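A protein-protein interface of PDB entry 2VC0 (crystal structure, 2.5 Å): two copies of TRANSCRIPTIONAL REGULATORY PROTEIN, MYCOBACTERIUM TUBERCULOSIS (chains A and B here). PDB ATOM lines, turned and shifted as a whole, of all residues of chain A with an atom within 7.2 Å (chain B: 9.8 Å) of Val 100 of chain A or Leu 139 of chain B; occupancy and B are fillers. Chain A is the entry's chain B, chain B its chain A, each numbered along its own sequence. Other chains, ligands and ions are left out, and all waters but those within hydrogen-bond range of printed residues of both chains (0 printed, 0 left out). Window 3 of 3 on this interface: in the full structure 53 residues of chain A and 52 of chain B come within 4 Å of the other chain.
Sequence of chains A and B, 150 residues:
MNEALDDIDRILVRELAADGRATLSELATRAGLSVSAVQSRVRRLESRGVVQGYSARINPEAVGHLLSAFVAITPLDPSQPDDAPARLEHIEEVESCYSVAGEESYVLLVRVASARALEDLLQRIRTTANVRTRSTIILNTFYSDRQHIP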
ATOM      1  N   ALA A  72       8.845 -11.110  -2.646  1.00  0.00           N
ATOM      2  CA  ALA A  72      10.182 -10.895  -2.128  1.00  0.00           C
ATOM      3  C   ALA A  72      10.837 -12.274  -2.025  1.00  0.00           C
ATOM      4  O   ALA A  72      10.242 -13.186  -1.420  1.00  0.00           O
ATOM      5  CB  ALA A  72      10.070 -10.259  -0.783  1.00  0.00           C
ATOM      6  N   ILE A  73      12.059 -12.438  -2.552  1.00  0.00           N
ATOM      7  CA  ILE A  73      12.720 -13.757  -2.536  1.00  0.00           C
ATOM      8  C   ILE A  73      14.145 -13.751  -1.951  1.00  0.00           C
ATOM      9  O   ILE A  73      14.924 -12.783  -2.060  1.00  0.00           O
ATOM     10  CB  ILE A  73      12.747 -14.468  -3.958  1.00  0.00           C
ATOM     11  CG1 ILE A  73      13.471 -13.630  -5.012  1.00  0.00           C
ATOM     12  CG2 ILE A  73      11.370 -14.715  -4.536  1.00  0.00           C
ATOM     13  CD1 ILE A  73      13.938 -14.454  -6.250  1.00  0.00           C
ATOM     14  N   TYR A  98      14.317  -7.100  -9.255  1.00  0.00           N
ATOM     15  CA  TYR A  98      15.210  -6.111  -8.684  1.00  0.00           C
ATOM     16  C   TYR A  98      15.980  -6.772  -7.564  1.00  0.00           C
ATOM     17  O   TYR A  98      15.420  -7.620  -6.832  1.00  0.00           O
ATOM     18  CB  TYR A  98      14.410  -5.014  -8.056  1.00  0.00           C
ATOM     19  CG  TYR A  98      13.430  -4.292  -8.944  1.00  0.00           C
ATOM     20  CD1 TYR A  98      12.044  -4.645  -8.994  1.00  0.00           C
ATOM     21  CD2 TYR A  98      13.859  -3.182  -9.730  1.00  0.00           C
ATOM     22  CE1 TYR A  98      11.091  -3.870  -9.821  1.00  0.00           C
ATOM     23  CE2 TYR A  98      12.951  -2.419 -10.567  1.00  0.00           C
ATOM     24  CZ  TYR A  98      11.604  -2.772 -10.611  1.00  0.00           C
ATOM     25  OH  TYR A  98      10.829  -2.037 -11.459  1.00  0.00           O
ATOM     26  N   SER A  99      17.266  -6.417  -7.409  1.00  0.00           N
ATOM     27  CA  SER A  99      17.989  -6.817  -6.177  1.00  0.00           C
ATOM     28  C   SER A  99      17.830  -5.659  -5.286  1.00  0.00           C
ATOM     29  O   SER A  99      17.624  -4.538  -5.734  1.00  0.00           O
ATOM     30  CB  SER A  99      19.468  -7.110  -6.379  1.00  0.00           C
ATOM     31  OG  SER A  99      20.039  -5.997  -7.051  1.00  0.00           O
ATOM     32  N   VAL A 100      17.902  -5.907  -3.998  1.00  0.00           N
ATOM     33  CA  VAL A 100      17.357  -4.889  -3.089  1.00  0.00           C
ATOM     34  C   VAL A 100      18.201  -4.905  -1.803  1.00  0.00           C
ATOM     35  O   VAL A 100      18.892  -5.904  -1.561  1.00  0.00           O
ATOM     36  CB  VAL A 100      15.886  -5.266  -2.991  1.00  0.00           C
ATOM     37  CG1 VAL A 100      15.512  -5.924  -1.711  1.00  0.00           C
ATOM     38  CG2 VAL A 100      14.965  -4.270  -3.709  1.00  0.00           C
ATOM     39  N   ALA A 101      18.242  -3.822  -1.040  1.00  0.00           N
ATOM     40  CA  ALA A 101      18.845  -3.885   0.301  1.00  0.00           C
ATOM     41  C   ALA A 101      17.757  -3.824   1.308  1.00  0.00           C
ATOM     42  O   ALA A 101      17.280  -2.728   1.628  1.00  0.00           O
ATOM     43  CB  ALA A 101      19.818  -2.727   0.563  1.00  0.00           C
ATOM     44  N   GLY A 102      17.309  -4.984   1.796  1.00  0.00           N
ATOM     45  CA  GLY A 102      16.418  -5.044   2.946  1.00  0.00           C
ATOM     46  C   GLY A 102      16.485  -6.379   3.591  1.00  0.00           C
ATOM     47  O   GLY A 102      17.576  -6.812   3.960  1.00  0.00           O
ATOM     48  N   GLU A 103      15.321  -7.045   3.729  1.00  0.00           N
ATOM     49  CA  GLU A 103      15.316  -8.387   4.357  1.00  0.00           C
ATOM     50  C   GLU A 103      15.551  -9.518   3.394  1.00  0.00           C
ATOM     51  O   GLU A 103      16.083 -10.542   3.762  1.00  0.00           O
ATOM     52  CB  GLU A 103      14.020  -8.699   5.045  1.00  0.00           C
ATOM     53  CG  GLU A 103      13.392  -7.522   5.714  1.00  0.00           C
ATOM     54  CD  GLU A 103      12.623  -7.980   6.971  1.00  0.00           C
ATOM     55  OE1 GLU A 103      12.682  -9.206   7.317  1.00  0.00           O
ATOM     56  OE2 GLU A 103      12.021  -7.093   7.609  1.00  0.00           O
ATOM     57  N   GLU A 104      15.043  -9.330   2.197  1.00  0.00           N
ATOM     58  CA  GLU A 104      15.084 -10.279   1.117  1.00  0.00           C
ATOM     59  C   GLU A 104      16.174  -9.848   0.158  1.00  0.00           C
ATOM     60  O   GLU A 104      16.621  -8.768   0.239  1.00  0.00           O
ATOM     61  CB  GLU A 104      13.737 -10.297   0.371  1.00  0.00           C
ATOM     62  CG  GLU A 104      12.550 -10.637   1.295  1.00  0.00           C
ATOM     63  CD  GLU A 104      12.617 -11.989   2.090  1.00  0.00           C
ATOM     64  OE1 GLU A 104      12.027 -11.970   3.240  1.00  0.00           O
ATOM     65  OE2 GLU A 104      13.164 -13.038   1.557  1.00  0.00           O
ATOM     66  N   SER A 105      16.590 -10.726  -0.727  1.00  0.00           N
ATOM     67  CA  SER A 105      17.603 -10.453  -1.736  1.00  0.00           C
ATOM     68  C   SER A 105      17.024  -9.804  -2.987  1.00  0.00           C
ATOM     69  O   SER A 105      17.691  -8.970  -3.532  1.00  0.00           O
ATOM     70  CB  SER A 105      18.312 -11.755  -2.154  1.00  0.00           C
ATOM     71  OG  SER A 105      18.916 -12.342  -1.014  1.00  0.00           O
ATOM     72  N   TYR A 106      15.809 -10.180  -3.425  1.00  0.00           N
ATOM     73  CA  TYR A 106      15.261  -9.615  -4.618  1.00  0.00           C
ATOM     74  C   TYR A 106      13.778  -9.329  -4.433  1.00  0.00           C
ATOM     75  O   TYR A 106      13.169  -9.969  -3.618  1.00  0.00           O
ATOM     76  CB  TYR A 106      15.372 -10.568  -5.805  1.00  0.00           C
ATOM     77  CG  TYR A 106      16.751 -11.031  -6.089  1.00  0.00           C
ATOM     78  CD1 TYR A 106      17.602 -10.304  -6.950  1.00  0.00           C
ATOM     79  CD2 TYR A 106      17.217 -12.248  -5.532  1.00  0.00           C
ATOM     80  CE1 TYR A 106      18.902 -10.807  -7.237  1.00  0.00           C
ATOM     81  CE2 TYR A 106      18.486 -12.708  -5.753  1.00  0.00           C
ATOM     82  CZ  TYR A 106      19.318 -11.980  -6.613  1.00  0.00           C
ATOM     83  OH  TYR A 106      20.578 -12.485  -6.847  1.00  0.00           O
ATOM     84  N   VAL A 107      13.206  -8.464  -5.275  1.00  0.00           N
ATOM     85  CA  VAL A 107      11.853  -8.250  -5.311  1.00  0.00           C
ATOM     86  C   VAL A 107      11.381  -8.421  -6.774  1.00  0.00           C
ATOM     87  O   VAL A 107      12.009  -7.826  -7.693  1.00  0.00           O
ATOM     88  CB  VAL A 107      11.544  -6.826  -4.841  1.00  0.00           C
ATOM     89  CG1 VAL A 107      10.050  -6.474  -5.106  1.00  0.00           C
ATOM     90  CG2 VAL A 107      11.858  -6.691  -3.409  1.00  0.00           C
ATOM     91  N   GLU B  61      19.280   6.078 -14.923  1.00  0.00           N
ATOM     92  CA  GLU B  61      20.674   6.528 -14.737  1.00  0.00           C
ATOM     93  C   GLU B  61      21.185   7.592 -15.681  1.00  0.00           C
ATOM     94  O   GLU B  61      21.792   8.563 -15.215  1.00  0.00           O
ATOM     95  CB  GLU B  61      21.651   5.399 -14.713  1.00  0.00           C
ATOM     96  CG  GLU B  61      21.804   4.903 -13.332  1.00  0.00           C
ATOM     97  CD  GLU B  61      22.041   3.407 -13.260  1.00  0.00           C
ATOM     98  OE1 GLU B  61      22.648   2.869 -14.213  1.00  0.00           O
ATOM     99  OE2 GLU B  61      21.636   2.786 -12.236  1.00  0.00           O
ATOM    100  N   HIS B  65      18.869   9.974 -12.076  1.00  0.00           N
ATOM    101  CA  HIS B  65      18.322   9.145 -11.029  1.00  0.00           C
ATOM    102  C   HIS B  65      19.225   7.976 -10.771  1.00  0.00           C
ATOM    103  O   HIS B  65      19.058   6.896 -11.323  1.00  0.00           O
ATOM    104  CB  HIS B  65      16.935   8.689 -11.406  1.00  0.00           C
ATOM    105  CG  HIS B  65      15.988   9.833 -11.676  1.00  0.00           C
ATOM    106  ND1 HIS B  65      15.972  10.986 -10.908  1.00  0.00           N
ATOM    107  CD2 HIS B  65      15.004   9.979 -12.606  1.00  0.00           C
ATOM    108  CE1 HIS B  65      15.016  11.786 -11.351  1.00  0.00           C
ATOM    109  NE2 HIS B  65      14.434  11.209 -12.397  1.00  0.00           N
ATOM    110  N   LEU B  66      20.198   8.227  -9.910  1.00  0.00           N
ATOM    111  CA  LEU B  66      21.148   7.241  -9.534  1.00  0.00           C
ATOM    112  C   LEU B  66      20.709   6.342  -8.391  1.00  0.00           C
ATOM    113  O   LEU B  66      21.308   5.319  -8.199  1.00  0.00           O
ATOM    114  CB  LEU B  66      22.417   7.969  -9.180  1.00  0.00           C
ATOM    115  CG  LEU B  66      23.026   8.637 -10.430  1.00  0.00           C
ATOM    116  CD1 LEU B  66      24.061   9.729 -10.046  1.00  0.00           C
ATOM    117  CD2 LEU B  66      23.616   7.482 -11.326  1.00  0.00           C
ATOM    118  N   LEU B  67      19.632   6.703  -7.668  1.00  0.00           N
ATOM    119  CA  LEU B  67      19.147   5.889  -6.569  1.00  0.00           C
ATOM    120  C   LEU B  67      17.655   5.677  -6.735  1.00  0.00           C
ATOM    121  O   LEU B  67      16.934   6.626  -6.894  1.00  0.00           O
ATOM    122  CB  LEU B  67      19.376   6.602  -5.231  1.00  0.00           C
ATOM    123  CG  LEU B  67      20.016   5.897  -4.017  1.00  0.00           C
ATOM    124  CD1 LEU B  67      19.894   6.741  -2.756  1.00  0.00           C
ATOM    125  CD2 LEU B  67      19.331   4.716  -3.711  1.00  0.00           C
ATOM    126  N   SER B  68      17.193   4.456  -6.553  1.00  0.00           N
ATOM    127  CA  SER B  68      15.791   4.141  -6.633  1.00  0.00           C
ATOM    128  C   SER B  68      15.445   3.370  -5.423  1.00  0.00           C
ATOM    129  O   SER B  68      16.277   2.613  -4.963  1.00  0.00           O
ATOM    130  CB  SER B  68      15.556   3.226  -7.812  1.00  0.00           C
ATOM    131  OG  SER B  68      15.432   4.073  -8.911  1.00  0.00           O
ATOM    132  N   ALA B  69      14.224   3.523  -4.939  1.00  0.00           N
ATOM    133  CA  ALA B  69      13.827   2.800  -3.744  1.00  0.00           C
ATOM    134  C   ALA B  69      12.334   2.460  -3.743  1.00  0.00           C
ATOM    135  O   ALA B  69      11.537   3.150  -4.379  1.00  0.00           O
ATOM    136  CB  ALA B  69      14.218   3.589  -2.465  1.00  0.00           C
ATOM    137  N   PHE B  70      11.977   1.363  -3.107  1.00  0.00           N
ATOM    138  CA  PHE B  70      10.582   1.120  -2.775  1.00  0.00           C
ATOM    139  C   PHE B  70      10.340   1.768  -1.391  1.00  0.00           C
ATOM    140  O   PHE B  70      11.147   1.561  -0.416  1.00  0.00           O
ATOM    141  CB  PHE B  70      10.312  -0.377  -2.649  1.00  0.00           C
ATOM    142  CG  PHE B  70      10.256  -1.087  -3.952  1.00  0.00           C
ATOM    143  CD1 PHE B  70      11.279  -1.995  -4.313  1.00  0.00           C
ATOM    144  CD2 PHE B  70       9.227  -0.831  -4.843  1.00  0.00           C
ATOM    145  CE1 PHE B  70      11.242  -2.638  -5.517  1.00  0.00           C
ATOM    146  CE2 PHE B  70       9.179  -1.432  -6.094  1.00  0.00           C
ATOM    147  CZ  PHE B  70      10.199  -2.373  -6.441  1.00  0.00           C
ATOM    148  N   VAL B  71       9.258   2.532  -1.278  1.00  0.00           N
ATOM    149  CA  VAL B  71       8.899   2.980   0.040  1.00  0.00           C
ATOM    150  C   VAL B  71       7.493   2.536   0.442  1.00  0.00           C
ATOM    151  O   VAL B  71       6.477   2.854  -0.233  1.00  0.00           O
ATOM    152  CB  VAL B  71       9.405   4.476   0.366  1.00  0.00           C
ATOM    153  CG1 VAL B  71      10.165   5.105  -0.738  1.00  0.00           C
ATOM    154  CG2 VAL B  71       8.381   5.396   0.987  1.00  0.00           C
ATOM    155  N   LEU B 109       7.202   3.535  -5.639  1.00  0.00           N
ATOM    156  CA  LEU B 109       8.533   3.466  -6.217  1.00  0.00           C
ATOM    157  C   LEU B 109       8.993   4.896  -6.472  1.00  0.00           C
ATOM    158  O   LEU B 109       8.296   5.733  -7.065  1.00  0.00           O
ATOM    159  CB  LEU B 109       8.530   2.647  -7.480  1.00  0.00           C
ATOM    160  CG  LEU B 109       9.771   2.736  -8.393  1.00  0.00           C
ATOM    161  CD1 LEU B 109      10.805   1.921  -7.893  1.00  0.00           C
ATOM    162  CD2 LEU B 109       9.406   2.136  -9.724  1.00  0.00           C
ATOM    163  N   ARG B 111      12.357   7.707  -7.316  1.00  0.00           N
ATOM    164  CA  ARG B 111      13.731   7.858  -7.916  1.00  0.00           C
ATOM    165  C   ARG B 111      14.385   9.187  -7.653  1.00  0.00           C
ATOM    166  O   ARG B 111      13.781  10.238  -7.864  1.00  0.00           O
ATOM    167  CB  ARG B 111      13.782   7.627  -9.442  1.00  0.00           C
ATOM    168  CG  ARG B 111      12.990   6.453  -9.879  1.00  0.00           C
ATOM    169  CD  ARG B 111      13.645   5.796 -10.985  1.00  0.00           C
ATOM    170  NE  ARG B 111      12.746   4.827 -11.596  1.00  0.00           N
ATOM    171  CZ  ARG B 111      12.940   3.506 -11.692  1.00  0.00           C
ATOM    172  NH1 ARG B 111      14.006   2.875 -11.171  1.00  0.00           N
ATOM    173  NH2 ARG B 111      12.017   2.812 -12.306  1.00  0.00           N
ATOM    174  N   ARG B 134       8.825   2.931   5.244  1.00  0.00           N
ATOM    175  CA  ARG B 134       9.874   1.861   5.407  1.00  0.00           C
ATOM    176  C   ARG B 134      10.504   1.769   4.036  1.00  0.00           C
ATOM    177  O   ARG B 134       9.806   1.719   3.006  1.00  0.00           O
ATOM    178  CB  ARG B 134       9.270   0.559   5.928  1.00  0.00           C
ATOM    179  CG  ARG B 134      10.130  -0.716   5.683  1.00  0.00           C
ATOM    180  CD  ARG B 134       9.518  -2.041   6.309  1.00  0.00           C
ATOM    181  NE  ARG B 134       8.342  -2.441   5.522  1.00  0.00           N
ATOM    182  CZ  ARG B 134       8.423  -3.118   4.351  1.00  0.00           C
ATOM    183  NH1 ARG B 134       9.621  -3.503   3.913  1.00  0.00           N
ATOM    184  NH2 ARG B 134       7.329  -3.411   3.608  1.00  0.00           N
ATOM    185  N   SER B 135      11.802   1.904   3.970  1.00  0.00           N
ATOM    186  CA  SER B 135      12.469   2.107   2.650  1.00  0.00           C
ATOM    187  C   SER B 135      13.238   0.939   2.265  1.00  0.00           C
ATOM    188  O   SER B 135      13.971   0.493   3.095  1.00  0.00           O
ATOM    189  CB  SER B 135      13.465   3.244   2.717  1.00  0.00           C
ATOM    190  OG  SER B 135      12.640   4.354   2.777  1.00  0.00           O
ATOM    191  N   THR B 136      13.129   0.509   1.006  1.00  0.00           N
ATOM    192  CA  THR B 136      13.971  -0.588   0.460  1.00  0.00           C
ATOM    193  C   THR B 136      14.701  -0.070  -0.749  1.00  0.00           C
ATOM    194  O   THR B 136      14.094   0.188  -1.813  1.00  0.00           O
ATOM    195  CB  THR B 136      13.118  -1.853   0.184  1.00  0.00           C
ATOM    196  OG1 THR B 136      12.464  -2.163   1.419  1.00  0.00           O
ATOM    197  CG2 THR B 136      13.961  -3.067  -0.137  1.00  0.00           C
ATOM    198  N   ILE B 137      15.975   0.263  -0.549  1.00  0.00           N
ATOM    199  CA  ILE B 137      16.794   0.712  -1.695  1.00  0.00           C
ATOM    200  C   ILE B 137      16.946  -0.385  -2.742  1.00  0.00           C
ATOM    201  O   ILE B 137      17.218  -1.509  -2.394  1.00  0.00           O
ATOM    202  CB  ILE B 137      18.264   1.110  -1.277  1.00  0.00           C
ATOM    203  CG1 ILE B 137      18.305   2.255  -0.227  1.00  0.00           C
ATOM    204  CG2 ILE B 137      19.125   1.456  -2.452  1.00  0.00           C
ATOM    205  CD1 ILE B 137      17.347   3.208  -0.348  1.00  0.00           C
ATOM    206  N   ILE B 138      16.842  -0.033  -4.017  1.00  0.00           N
ATOM    207  CA  ILE B 138      17.061  -0.973  -5.097  1.00  0.00           C
ATOM    208  C   ILE B 138      18.541  -0.943  -5.476  1.00  0.00           C
ATOM    209  O   ILE B 138      19.076   0.141  -5.570  1.00  0.00           O
ATOM    210  CB  ILE B 138      16.218  -0.575  -6.284  1.00  0.00           C
ATOM    211  CG1 ILE B 138      14.756  -0.817  -5.918  1.00  0.00           C
ATOM    212  CG2 ILE B 138      16.677  -1.363  -7.566  1.00  0.00           C
ATOM    213  CD1 ILE B 138      13.795  -0.280  -6.999  1.00  0.00           C
ATOM    214  N   LEU B 139      19.213  -2.083  -5.594  1.00  0.00           N
ATOM    215  CA  LEU B 139      20.653  -2.049  -5.887  1.00  0.00           C
ATOM    216  C   LEU B 139      20.859  -2.153  -7.421  1.00  0.00           C
ATOM    217  O   LEU B 139      21.757  -1.488  -7.978  1.00  0.00           O
ATOM    218  CB  LEU B 139      21.436  -3.166  -5.193  1.00  0.00           C
ATOM    219  CG  LEU B 139      21.243  -3.184  -3.663  1.00  0.00           C
ATOM    220  CD1 LEU B 139      21.802  -4.394  -2.995  1.00  0.00           C
ATOM    221  CD2 LEU B 139      21.829  -1.939  -2.999  1.00  0.00           C
ATOM    222  N   ASN B 140      20.015  -2.954  -8.091  1.00  0.00           N
ATOM    223  CA  ASN B 140      20.110  -3.200  -9.473  1.00  0.00           C
ATOM    224  C   ASN B 140      18.752  -3.674 -10.085  1.00  0.00           C
ATOM    225  O   ASN B 140      18.012  -4.422  -9.460  1.00  0.00           O
ATOM    226  CB  ASN B 140      21.197  -4.244  -9.687  1.00  0.00           C
ATOM    227  CG  ASN B 140      21.438  -4.534 -11.209  1.00  0.00           C
ATOM    228  OD1 ASN B 140      21.370  -3.637 -12.054  1.00  0.00           O
ATOM    229  ND2 ASN B 140      21.621  -5.801 -11.535  1.00  0.00           N
ATOM    230  N   THR B 141      18.426  -3.236 -11.304  1.00  0.00           N
ATOM    231  CA  THR B 141      17.222  -3.630 -12.004  1.00  0.00           C
ATOM    232  C   THR B 141      17.668  -4.647 -13.029  1.00  0.00           C
ATOM    233  O   THR B 141      18.401  -4.298 -13.913  1.00  0.00           O
ATOM    234  CB  THR B 141      16.705  -2.488 -12.725  1.00  0.00           C
ATOM    235  OG1 THR B 141      16.254  -1.565 -11.737  1.00  0.00           O
ATOM    236  CG2 THR B 141      15.486  -2.831 -13.457  1.00  0.00           C
ATOM    237  N   PHE B 142      17.293  -5.914 -12.908  1.00  0.00           N
ATOM    238  CA  PHE B 142      17.642  -6.890 -13.907  1.00  0.00           C
ATOM    239  C   PHE B 142      16.783  -6.813 -15.145  1.00  0.00           C
ATOM    240  O   PHE B 142      17.263  -7.077 -16.231  1.00  0.00           O
ATOM    241  CB  PHE B 142      17.550  -8.269 -13.294  1.00  0.00           C
ATOM    242  CG  PHE B 142      18.616  -8.492 -12.274  1.00  0.00           C
ATOM    243  CD1 PHE B 142      19.849  -9.059 -12.660  1.00  0.00           C
ATOM    244  CD2 PHE B 142      18.441  -8.005 -10.922  1.00  0.00           C
ATOM    245  CE1 PHE B 142      20.913  -9.202 -11.673  1.00  0.00           C
ATOM    246  CE2 PHE B 142      19.466  -8.143  -9.971  1.00  0.00           C
ATOM    247  CZ  PHE B 142      20.721  -8.760 -10.350  1.00  0.00           C
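The backbone NH (N) of Ala 101 of chain A is in hydrogen-bond range of the backbone carbonyl oxygen (O) of Ile 137 of chain B.
The backbone NH (N) of Leu 139 of chain B is in hydrogen-bond range of the backbone carbonyl oxygen (O) of Ser 99 of chain A.
N of Ser 99 of chain A is in hydrogen-bond range of O of Asn 140 of chain B (3.0 Å).
The backbone carbonyl oxygen of Ser 68 of chain B is in hydrogen-bond range of the backbone NH of Ile 138 of chain B (2.9 Å).
The backbone NH (N) of Thr 136 of chain B is in hydrogen-bond range of the backbone carbonyl oxygen (O) of Phe 70 of chain B, 2.7 Å away.
The backbone carbonyl oxygen of Tyr 106 of chain A lies within hydrogen-bond range of the backbone NH of Ile 73 of chain A.
The backbone carbonyl oxygen of Tyr 98 of chain A sits at hydrogen-bond distance from the backbone NH of Val 107 of chain A.
The backbone NH (N) of Val 100 of chain A lies within hydrogen-bond range of the backbone carbonyl oxygen (O) of Ser 105 of chain A, at 3.1 Å.
Among the printed residues, merely in contact across the chains: Tyr 98 of chain A with Asn 140 of chain B (3.4 Å), Val 100 of chain A with Ile 137 of chain B (3.5 Å), Tyr 98 of chain A with Thr 141 of chain B (3.5 Å), Val 100 of chain A with Leu 139 of chain B (3.6 Å), Val 100 of chain A with Thr 136 of chain B (3.6 Å), Ser 99 of chain A with Ile 138 of chain B (3.7 Å), Ser 99 of chain A with Phe 142 of chain B (3.7 Å), Ala 101 of chain A with Thr 136 of chain B (3.8 Å), Tyr 98 of chain A with Phe 70 of chain B (3.8 Å), Tyr 106 of chain A with Phe 142 of chain B (3.9 Å) and Tyr 98 of chain A with Ile 138 of chain B (3.99 Å).
Val 100 of chain A touches just these residues of chain B: Thr 136 (3.6 Å), Ile 137 (3.5 Å) and Leu 139 (3.6 Å).
Of the printed residues of chain A, Leu 139 of chain B touches Ser 99 (2.9 Å) and Val 100 (3.6 Å).
Of chain B, only Ile 138, Leu 139, Asn 140 and Phe 142 come within 4 Å of Ser 99 of chain A.
Ala 101 of chain A touches just these residues of chain B: Thr 136 and Ile 137.
No residue of chain B comes within 4 Å of Gly 102 of chain A.
Printed residues of chain B within 4 Å of Tyr 106 of chain A: Phe 142.
Printed residues of chain A within 4 Å of Ile 138 of chain B: Tyr 98 (3.99 Å) and Ser 99 (3.7 Å).
Glu 103 of chain A touches none of the printed residues of chain B.
Ser 68 of chain B touches none of the printed residues of chain A.
The nearest residue of chain A that does not touch Leu 139 of chain B is Ala 101 of chain A (4.04 Å).
Hydrophobic or aromatic side chains of chain A within 4 Å of the printed part of chain B: Tyr 98, Val 100 and Tyr 106.
Along chain A the printed residues that touch a printed residue of chain B span positions 98 to 106.
Printed residues of chain B that touch a printed residue of chain A: Phe 70, Thr 136, Ile 137, Ile 138, Leu 139, Asn 140, Thr 141 and Phe 142.
No position is printed for both chains.
Of the 14 pairs that touch across the chains among the printed residues, none has its exchanged pair printed and touching as well.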
